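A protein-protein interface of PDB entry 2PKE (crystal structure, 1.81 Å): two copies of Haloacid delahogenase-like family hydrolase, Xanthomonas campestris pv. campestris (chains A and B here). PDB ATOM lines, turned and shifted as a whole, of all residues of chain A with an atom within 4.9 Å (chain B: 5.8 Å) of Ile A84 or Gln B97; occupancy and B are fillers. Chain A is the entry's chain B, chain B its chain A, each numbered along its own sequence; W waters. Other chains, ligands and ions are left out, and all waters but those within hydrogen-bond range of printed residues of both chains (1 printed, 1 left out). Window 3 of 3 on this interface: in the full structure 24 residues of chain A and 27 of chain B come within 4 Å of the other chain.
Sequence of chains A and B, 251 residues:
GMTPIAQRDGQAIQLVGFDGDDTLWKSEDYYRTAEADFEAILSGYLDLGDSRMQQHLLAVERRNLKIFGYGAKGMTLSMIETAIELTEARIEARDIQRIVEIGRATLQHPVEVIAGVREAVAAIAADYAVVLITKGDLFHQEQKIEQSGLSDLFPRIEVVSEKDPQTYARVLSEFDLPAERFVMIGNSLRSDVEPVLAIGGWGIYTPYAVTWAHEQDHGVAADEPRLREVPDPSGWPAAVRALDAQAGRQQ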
ATOM      1  N   ILE A  80     -14.244 -13.045 -19.144  1.00  0.00           N
ATOM      2  CA  ILE A  80     -13.147 -13.749 -18.485  1.00  0.00           C
ATOM      3  C   ILE A  80     -12.386 -14.695 -19.403  1.00  0.00           C
ATOM      4  O   ILE A  80     -11.143 -14.653 -19.445  1.00  0.00           O
ATOM      5  CB  ILE A  80     -13.634 -14.495 -17.198  1.00  0.00           C
ATOM      6  CG1 ILE A  80     -13.923 -13.483 -16.055  1.00  0.00           C
ATOM      7  CG2 ILE A  80     -12.573 -15.449 -16.719  1.00  0.00           C
ATOM      8  CD1 ILE A  80     -14.743 -14.050 -14.883  1.00  0.00           C
ATOM      9  N   GLU A  81     -13.100 -15.544 -20.123  1.00  0.00           N
ATOM     10  CA  GLU A  81     -12.450 -16.486 -21.047  1.00  0.00           C
ATOM     11  C   GLU A  81     -11.674 -15.721 -22.139  1.00  0.00           C
ATOM     12  O   GLU A  81     -10.560 -16.087 -22.510  1.00  0.00           O
ATOM     13  CB  GLU A  81     -13.496 -17.370 -21.727  1.00  0.00           C
ATOM     14  CG  GLU A  81     -14.038 -18.537 -20.912  1.00  0.00           C
ATOM     15  CD  GLU A  81     -14.622 -19.631 -21.826  1.00  0.00           C
ATOM     16  N   THR A  82     -12.307 -14.670 -22.662  1.00  0.00           N
ATOM     17  CA  THR A  82     -11.735 -13.856 -23.688  1.00  0.00           C
ATOM     18  C   THR A  82     -10.412 -13.281 -23.194  1.00  0.00           C
ATOM     19  O   THR A  82      -9.410 -13.438 -23.832  1.00  0.00           O
ATOM     20  CB  THR A  82     -12.682 -12.751 -24.060  1.00  0.00           C
ATOM     21  OG1 THR A  82     -13.842 -13.319 -24.687  1.00  0.00           O
ATOM     22  CG2 THR A  82     -12.023 -11.736 -24.995  1.00  0.00           C
ATOM     23  N   ALA A  83     -10.434 -12.607 -22.047  1.00  0.00           N
ATOM     24  CA  ALA A  83      -9.247 -12.019 -21.469  1.00  0.00           C
ATOM     25  C   ALA A  83      -8.181 -13.026 -21.290  1.00  0.00           C
ATOM     26  O   ALA A  83      -7.038 -12.729 -21.573  1.00  0.00           O
ATOM     27  CB  ALA A  83      -9.563 -11.396 -20.129  1.00  0.00           C
ATOM     28  N   ILE A  84      -8.516 -14.198 -20.761  1.00  0.00           N
ATOM     29  CA  ILE A  84      -7.516 -15.273 -20.577  1.00  0.00           C
ATOM     30  C   ILE A  84      -6.939 -15.749 -21.904  1.00  0.00           C
ATOM     31  O   ILE A  84      -5.725 -15.890 -22.041  1.00  0.00           O
ATOM     32  CB  ILE A  84      -8.097 -16.465 -19.773  1.00  0.00           C
ATOM     33  CG1 ILE A  84      -8.284 -16.025 -18.301  1.00  0.00           C
ATOM     34  CG2 ILE A  84      -7.200 -17.697 -19.897  1.00  0.00           C
ATOM     35  CD1 ILE A  84      -9.151 -16.925 -17.445  1.00  0.00           C
ATOM     36  N   GLU A  85      -7.805 -15.927 -22.889  1.00  0.00           N
ATOM     37  CA  GLU A  85      -7.391 -16.316 -24.229  1.00  0.00           C
ATOM     38  C   GLU A  85      -6.450 -15.262 -24.843  1.00  0.00           C
ATOM     39  O   GLU A  85      -5.290 -15.556 -25.150  1.00  0.00           O
ATOM     40  CB  GLU A  85      -8.614 -16.488 -25.089  1.00  0.00           C
ATOM     41  CG  GLU A  85      -8.468 -17.381 -26.263  1.00  0.00           C
ATOM     42  CD  GLU A  85      -9.842 -17.729 -26.844  1.00  0.00           C
ATOM     43  OE1 GLU A  85     -10.847 -17.778 -26.072  1.00  0.00           O
ATOM     44  OE2 GLU A  85      -9.921 -17.931 -28.073  1.00  0.00           O
ATOM     45  N   LEU A  86      -6.946 -14.030 -24.970  1.00  0.00           N
ATOM     46  CA  LEU A  86      -6.215 -12.939 -25.627  1.00  0.00           C
ATOM     47  C   LEU A  86      -4.895 -12.560 -24.977  1.00  0.00           C
ATOM     48  O   LEU A  86      -4.040 -12.002 -25.697  1.00  0.00           O
ATOM     49  CB  LEU A  86      -7.072 -11.677 -25.724  1.00  0.00           C
ATOM     50  CG  LEU A  86      -8.069 -11.536 -26.893  1.00  0.00           C
ATOM     51  CD1 LEU A  86      -8.640 -12.847 -27.327  1.00  0.00           C
ATOM     52  CD2 LEU A  86      -9.153 -10.558 -26.485  1.00  0.00           C
ATOM     53  N   THR A  87      -4.764 -12.781 -23.650  1.00  0.00           N
ATOM     54  CA  THR A  87      -3.519 -12.503 -22.902  1.00  0.00           C
ATOM     55  C   THR A  87      -2.629 -13.724 -22.733  1.00  0.00           C
ATOM     56  O   THR A  87      -1.584 -13.662 -22.044  1.00  0.00           O
ATOM     57  CB  THR A  87      -3.758 -11.859 -21.476  1.00  0.00           C
ATOM     58  OG1 THR A  87      -4.436 -12.773 -20.584  1.00  0.00           O
ATOM     59  CG2 THR A  87      -4.524 -10.533 -21.611  1.00  0.00           C
ATOM     60  N   GLU A  88      -3.007 -14.820 -23.390  1.00  0.00           N
ATOM     61  CA  GLU A  88      -2.230 -16.056 -23.322  1.00  0.00           C
ATOM     62  C   GLU A  88      -2.061 -16.448 -21.851  1.00  0.00           C
ATOM     63  O   GLU A  88      -0.992 -16.880 -21.403  1.00  0.00           O
ATOM     64  CB  GLU A  88      -0.925 -15.915 -24.148  1.00  0.00           C
ATOM     65  CG  GLU A  88      -1.211 -15.720 -25.676  1.00  0.00           C
ATOM     66  CD  GLU A  88      -0.001 -15.385 -26.537  1.00  0.00           C
ATOM     67  OE1 GLU A  88       0.829 -14.535 -26.147  1.00  0.00           O
ATOM     68  OE2 GLU A  88       0.115 -15.957 -27.648  1.00  0.00           O
ATOM     69  N   ALA A  89      -3.161 -16.272 -21.102  1.00  0.00           N
ATOM     70  CA  ALA A  89      -3.235 -16.551 -19.641  1.00  0.00           C
ATOM     71  C   ALA A  89      -2.203 -15.794 -18.761  1.00  0.00           C
ATOM     72  O   ALA A  89      -1.761 -16.290 -17.731  1.00  0.00           O
ATOM     73  CB  ALA A  89      -3.170 -18.065 -19.392  1.00  0.00           C
ATOM     74  N   ILE A  91      -2.961 -12.592 -17.821  1.00  0.00           N
ATOM     75  CA  ILE A  91      -3.802 -11.719 -17.002  1.00  0.00           C
ATOM     76  C   ILE A  91      -3.733 -12.159 -15.525  1.00  0.00           C
ATOM     77  O   ILE A  91      -3.710 -13.337 -15.205  1.00  0.00           O
ATOM     78  CB  ILE A  91      -5.241 -11.619 -17.560  1.00  0.00           C
ATOM     79  CG1 ILE A  91      -6.056 -10.577 -16.750  1.00  0.00           C
ATOM     80  CG2 ILE A  91      -5.911 -13.018 -17.615  1.00  0.00           C
ATOM     81  CD1 ILE A  91      -7.447 -10.278 -17.323  1.00  0.00           C
ATOM     82  N   ILE A  96      -8.799 -10.248 -13.275  1.00  0.00           N
ATOM     83  CA  ILE A  96      -9.990 -11.106 -13.414  1.00  0.00           C
ATOM     84  C   ILE A  96     -11.025 -10.740 -12.355  1.00  0.00           C
ATOM     85  O   ILE A  96     -12.211 -10.686 -12.639  1.00  0.00           O
ATOM     86  CB  ILE A  96      -9.635 -12.617 -13.337  1.00  0.00           C
ATOM     87  CG1 ILE A  96      -8.894 -13.013 -14.598  1.00  0.00           C
ATOM     88  CG2 ILE A  96     -10.892 -13.484 -13.167  1.00  0.00           C
ATOM     89  CD1 ILE A  96      -8.219 -14.314 -14.514  1.00  0.00           C
ATOM     90  N   GLU B  92      -3.291 -18.654 -10.920  1.00  0.00           N
ATOM     91  CA  GLU B  92      -3.036 -18.423 -12.340  1.00  0.00           C
ATOM     92  C   GLU B  92      -4.298 -18.282 -13.216  1.00  0.00           C
ATOM     93  O   GLU B  92      -5.262 -18.972 -13.002  1.00  0.00           O
ATOM     94  CB  GLU B  92      -2.186 -19.567 -12.880  1.00  0.00           C
ATOM     95  CG  GLU B  92      -0.744 -19.528 -12.381  1.00  0.00           C
ATOM     96  CD  GLU B  92      -0.007 -18.296 -12.815  1.00  0.00           C
ATOM     97  OE1 GLU B  92      -0.500 -17.567 -13.705  1.00  0.00           O
ATOM     98  OE2 GLU B  92       1.069 -18.058 -12.251  1.00  0.00           O
ATOM     99  N   ALA B  93      -4.259 -17.399 -14.223  1.00  0.00           N
ATOM    100  CA  ALA B  93      -5.347 -17.289 -15.209  1.00  0.00           C
ATOM    101  C   ALA B  93      -5.646 -18.664 -15.845  1.00  0.00           C
ATOM    102  O   ALA B  93      -6.793 -19.039 -16.046  1.00  0.00           O
ATOM    103  CB  ALA B  93      -4.983 -16.240 -16.294  1.00  0.00           C
ATOM    104  N   ARG B  94      -4.602 -19.458 -16.105  1.00  0.00           N
ATOM    105  CA  ARG B  94      -4.833 -20.809 -16.582  1.00  0.00           C
ATOM    106  C   ARG B  94      -5.746 -21.629 -15.634  1.00  0.00           C
ATOM    107  O   ARG B  94      -6.634 -22.366 -16.085  1.00  0.00           O
ATOM    108  CB  ARG B  94      -3.511 -21.538 -16.853  1.00  0.00           C
ATOM    109  CG  ARG B  94      -3.685 -22.953 -17.308  1.00  0.00           C
ATOM    110  CD  ARG B  94      -4.642 -23.095 -18.501  1.00  0.00           C
ATOM    111  NE  ARG B  94      -5.753 -24.041 -18.277  1.00  0.00           N
ATOM    112  N   ASP B  95      -5.563 -21.490 -14.330  1.00  0.00           N
ATOM    113  CA  ASP B  95      -6.413 -22.245 -13.383  1.00  0.00           C
ATOM    114  C   ASP B  95      -7.821 -21.646 -13.217  1.00  0.00           C
ATOM    115  O   ASP B  95      -8.809 -22.363 -12.997  1.00  0.00           O
ATOM    116  CB  ASP B  95      -5.695 -22.437 -12.059  1.00  0.00           C
ATOM    117  CG  ASP B  95      -4.594 -23.449 -12.156  1.00  0.00           C
ATOM    118  OD1 ASP B  95      -4.693 -24.386 -13.003  1.00  0.00           O
ATOM    119  OD2 ASP B  95      -3.609 -23.296 -11.399  1.00  0.00           O
ATOM    120  N   ILE B  96      -7.939 -20.344 -13.398  1.00  0.00           N
ATOM    121  CA  ILE B  96      -9.279 -19.714 -13.497  1.00  0.00           C
ATOM    122  C   ILE B  96     -10.024 -20.202 -14.730  1.00  0.00           C
ATOM    123  O   ILE B  96     -11.229 -20.423 -14.650  1.00  0.00           O
ATOM    124  CB  ILE B  96      -9.190 -18.180 -13.539  1.00  0.00           C
ATOM    125  CG1 ILE B  96      -8.602 -17.681 -12.236  1.00  0.00           C
ATOM    126  CG2 ILE B  96     -10.586 -17.555 -13.744  1.00  0.00           C
ATOM    127  CD1 ILE B  96      -9.525 -17.926 -11.065  1.00  0.00           C
ATOM    128  N   GLN B  97      -9.289 -20.346 -15.830  1.00  0.00           N
ATOM    129  CA  GLN B  97      -9.751 -21.005 -17.038  1.00  0.00           C
ATOM    130  C   GLN B  97     -10.376 -22.351 -16.693  1.00  0.00           C
ATOM    131  O   GLN B  97     -11.504 -22.652 -17.112  1.00  0.00           O
ATOM    132  CB  GLN B  97      -8.593 -21.217 -18.016  1.00  0.00           C
ATOM    133  CG  GLN B  97      -8.999 -21.826 -19.358  1.00  0.00           C
ATOM    134  CD  GLN B  97      -8.121 -21.330 -20.471  1.00  0.00           C
ATOM    135  OE1 GLN B  97      -6.907 -21.547 -20.460  1.00  0.00           O
ATOM    136  NE2 GLN B  97      -8.717 -20.631 -21.433  1.00  0.00           N
ATOM    137  N   ARG B  98      -9.637 -23.128 -15.899  1.00  0.00           N
ATOM    138  CA  ARG B  98     -10.081 -24.446 -15.424  1.00  0.00           C
ATOM    139  C   ARG B  98     -11.339 -24.404 -14.557  1.00  0.00           C
ATOM    140  O   ARG B  98     -12.171 -25.286 -14.617  1.00  0.00           O
ATOM    141  CB  ARG B  98      -8.925 -25.176 -14.704  1.00  0.00           C
ATOM    142  CG  ARG B  98      -8.035 -25.887 -15.659  1.00  0.00           C
ATOM    143  CD  ARG B  98      -6.647 -26.100 -15.173  1.00  0.00           C
ATOM    144  NE  ARG B  98      -6.504 -26.544 -13.789  1.00  0.00           N
ATOM    145  CZ  ARG B  98      -6.259 -27.789 -13.388  1.00  0.00           C
ATOM    146  NH1 ARG B  98      -6.198 -28.797 -14.248  1.00  0.00           N
ATOM    147  NH2 ARG B  98      -6.086 -28.038 -12.096  1.00  0.00           N
ATOM    148  N   ILE B  99     -11.499 -23.362 -13.765  1.00  0.00           N
ATOM    149  CA  ILE B  99     -12.738 -23.165 -13.018  1.00  0.00           C
ATOM    150  C   ILE B  99     -13.885 -22.862 -13.992  1.00  0.00           C
ATOM    151  O   ILE B  99     -14.987 -23.417 -13.848  1.00  0.00           O
ATOM    152  CB  ILE B  99     -12.599 -22.055 -12.011  1.00  0.00           C
ATOM    153  CG1 ILE B  99     -11.609 -22.480 -10.902  1.00  0.00           C
ATOM    154  CG2 ILE B  99     -13.970 -21.676 -11.414  1.00  0.00           C
ATOM    155  CD1 ILE B  99     -11.275 -21.390  -9.960  1.00  0.00           C
ATOM    156  N   VAL B 100     -13.656 -22.000 -14.984  1.00  0.00           N
ATOM    157  CA  VAL B 100     -14.715 -21.749 -15.972  1.00  0.00           C
ATOM    158  C   VAL B 100     -15.141 -23.070 -16.634  1.00  0.00           C
ATOM    159  O   VAL B 100     -16.323 -23.277 -16.865  1.00  0.00           O
ATOM    160  CB  VAL B 100     -14.308 -20.724 -17.055  1.00  0.00           C
ATOM    161  CG1 VAL B 100     -15.383 -20.670 -18.204  1.00  0.00           C
ATOM    162  CG2 VAL B 100     -14.028 -19.342 -16.413  1.00  0.00           C
ATOM    163  N   GLU B 101     -14.196 -23.952 -16.943  1.00  0.00           N
ATOM    164  CA  GLU B 101     -14.518 -25.258 -17.558  1.00  0.00           C
ATOM    165  C   GLU B 101     -15.336 -26.145 -16.656  1.00  0.00           C
ATOM    166  O   GLU B 101     -16.237 -26.817 -17.130  1.00  0.00           O
ATOM    167  CB  GLU B 101     -13.284 -26.028 -17.988  1.00  0.00           C
ATOM    168  CG  GLU B 101     -12.456 -25.314 -19.042  1.00  0.00           C
ATOM    169  CD  GLU B 101     -13.112 -25.268 -20.418  1.00  0.00           C
ATOM    170  OE1 GLU B 101     -14.200 -25.869 -20.606  1.00  0.00           O
ATOM    171  OE2 GLU B 101     -12.510 -24.627 -21.314  1.00  0.00           O
ATOM    172  N   ILE B 102     -15.045 -26.151 -15.363  1.00  0.00           N
ATOM    173  CA  ILE B 102     -15.905 -26.840 -14.412  1.00  0.00           C
ATOM    174  C   ILE B 102     -17.342 -26.384 -14.602  1.00  0.00           C
ATOM    175  O   ILE B 102     -18.282 -27.167 -14.631  1.00  0.00           O
ATOM    176  CB  ILE B 102     -15.519 -26.561 -12.941  1.00  0.00           C
ATOM    177  CG1 ILE B 102     -14.115 -27.065 -12.636  1.00  0.00           C
ATOM    178  CG2 ILE B 102     -16.510 -27.281 -12.002  1.00  0.00           C
ATOM    179  CD1 ILE B 102     -13.681 -26.759 -11.220  1.00  0.00           C
HETATM  180  O   HOH W   1      -1.772 -18.513 -16.283  1.00  0.00           O
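Water W1 lies within hydrogen-bond range of O of Ala A89 (2.7 Å), N of Arg B94 (3.0 Å), OE1 of Glu B92 (3.0 Å) and N of Ala B93 (3.4 Å).
Of the 11 printed residues of chain B, 4 touch a printed residue of chain A.
Of the 12 printed residues of chain A, 4 touch a printed residue of chain B.
Hydrophobic or aromatic side chains of chain A within 4 Å of the printed part of chain B: Ile A84, Ala A89 and Ile A91.
Among the printed residues, 6 pairs touch across the chains.
Of the printed residues of chain B, Ile A84 touches Ala B93 (3.5 Å) and Gln B97 (3.6 Å).
Of the printed residues of chain A, Gln B97 touches Ile A84.
Printed residues of chain A within 4 Å of Ala B93: Ile A84, Ala A89 and Ile A91.
Printed residues of chain B within 4 Å of Ile A91: Ala B93.
Of the printed residues of chain B, Ala A89 touches Ala B93 and Arg B94.
Of the printed residues of chain A, Val B100 touches Glu A81.
Of the printed residues of chain B, Glu A81 touches Val B100 (3.7 Å).
The nearest printed residue of chain B that does not touch Ile A84 is Ile B96 (4.02 Å).
The nearest printed residue of chain A that does not touch Gln B97 is Glu A85 (5.0 Å).
The nearest printed residue of chain B that does not touch Ala A89 is Glu B92 (4.4 Å).
Among the printed residues, pairs that only touch across the chains: Glu A81 with Val B100 (3.7 Å), Ile A84 with Ala B93 (3.5 Å), Ile A84 with Gln B97 (3.6 Å), Ala A89 with Ala B93 (3.5 Å), Ala A89 with Arg B94 (3.8 Å) and Ile A91 with Ala B93 (3.4 Å).
N of Ala A89 is in hydrogen-bond range of O of Ile A84 (2.8 Å).
The backbone NH of Ile A91 is in hydrogen-bond range of the side-chain hydroxyl of Thr A87 (3.1 Å).
Position printed for both chains: 96.
Of the 6 pairs that touch across the chains among the printed residues, none has its exchanged pair printed and touching as well.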
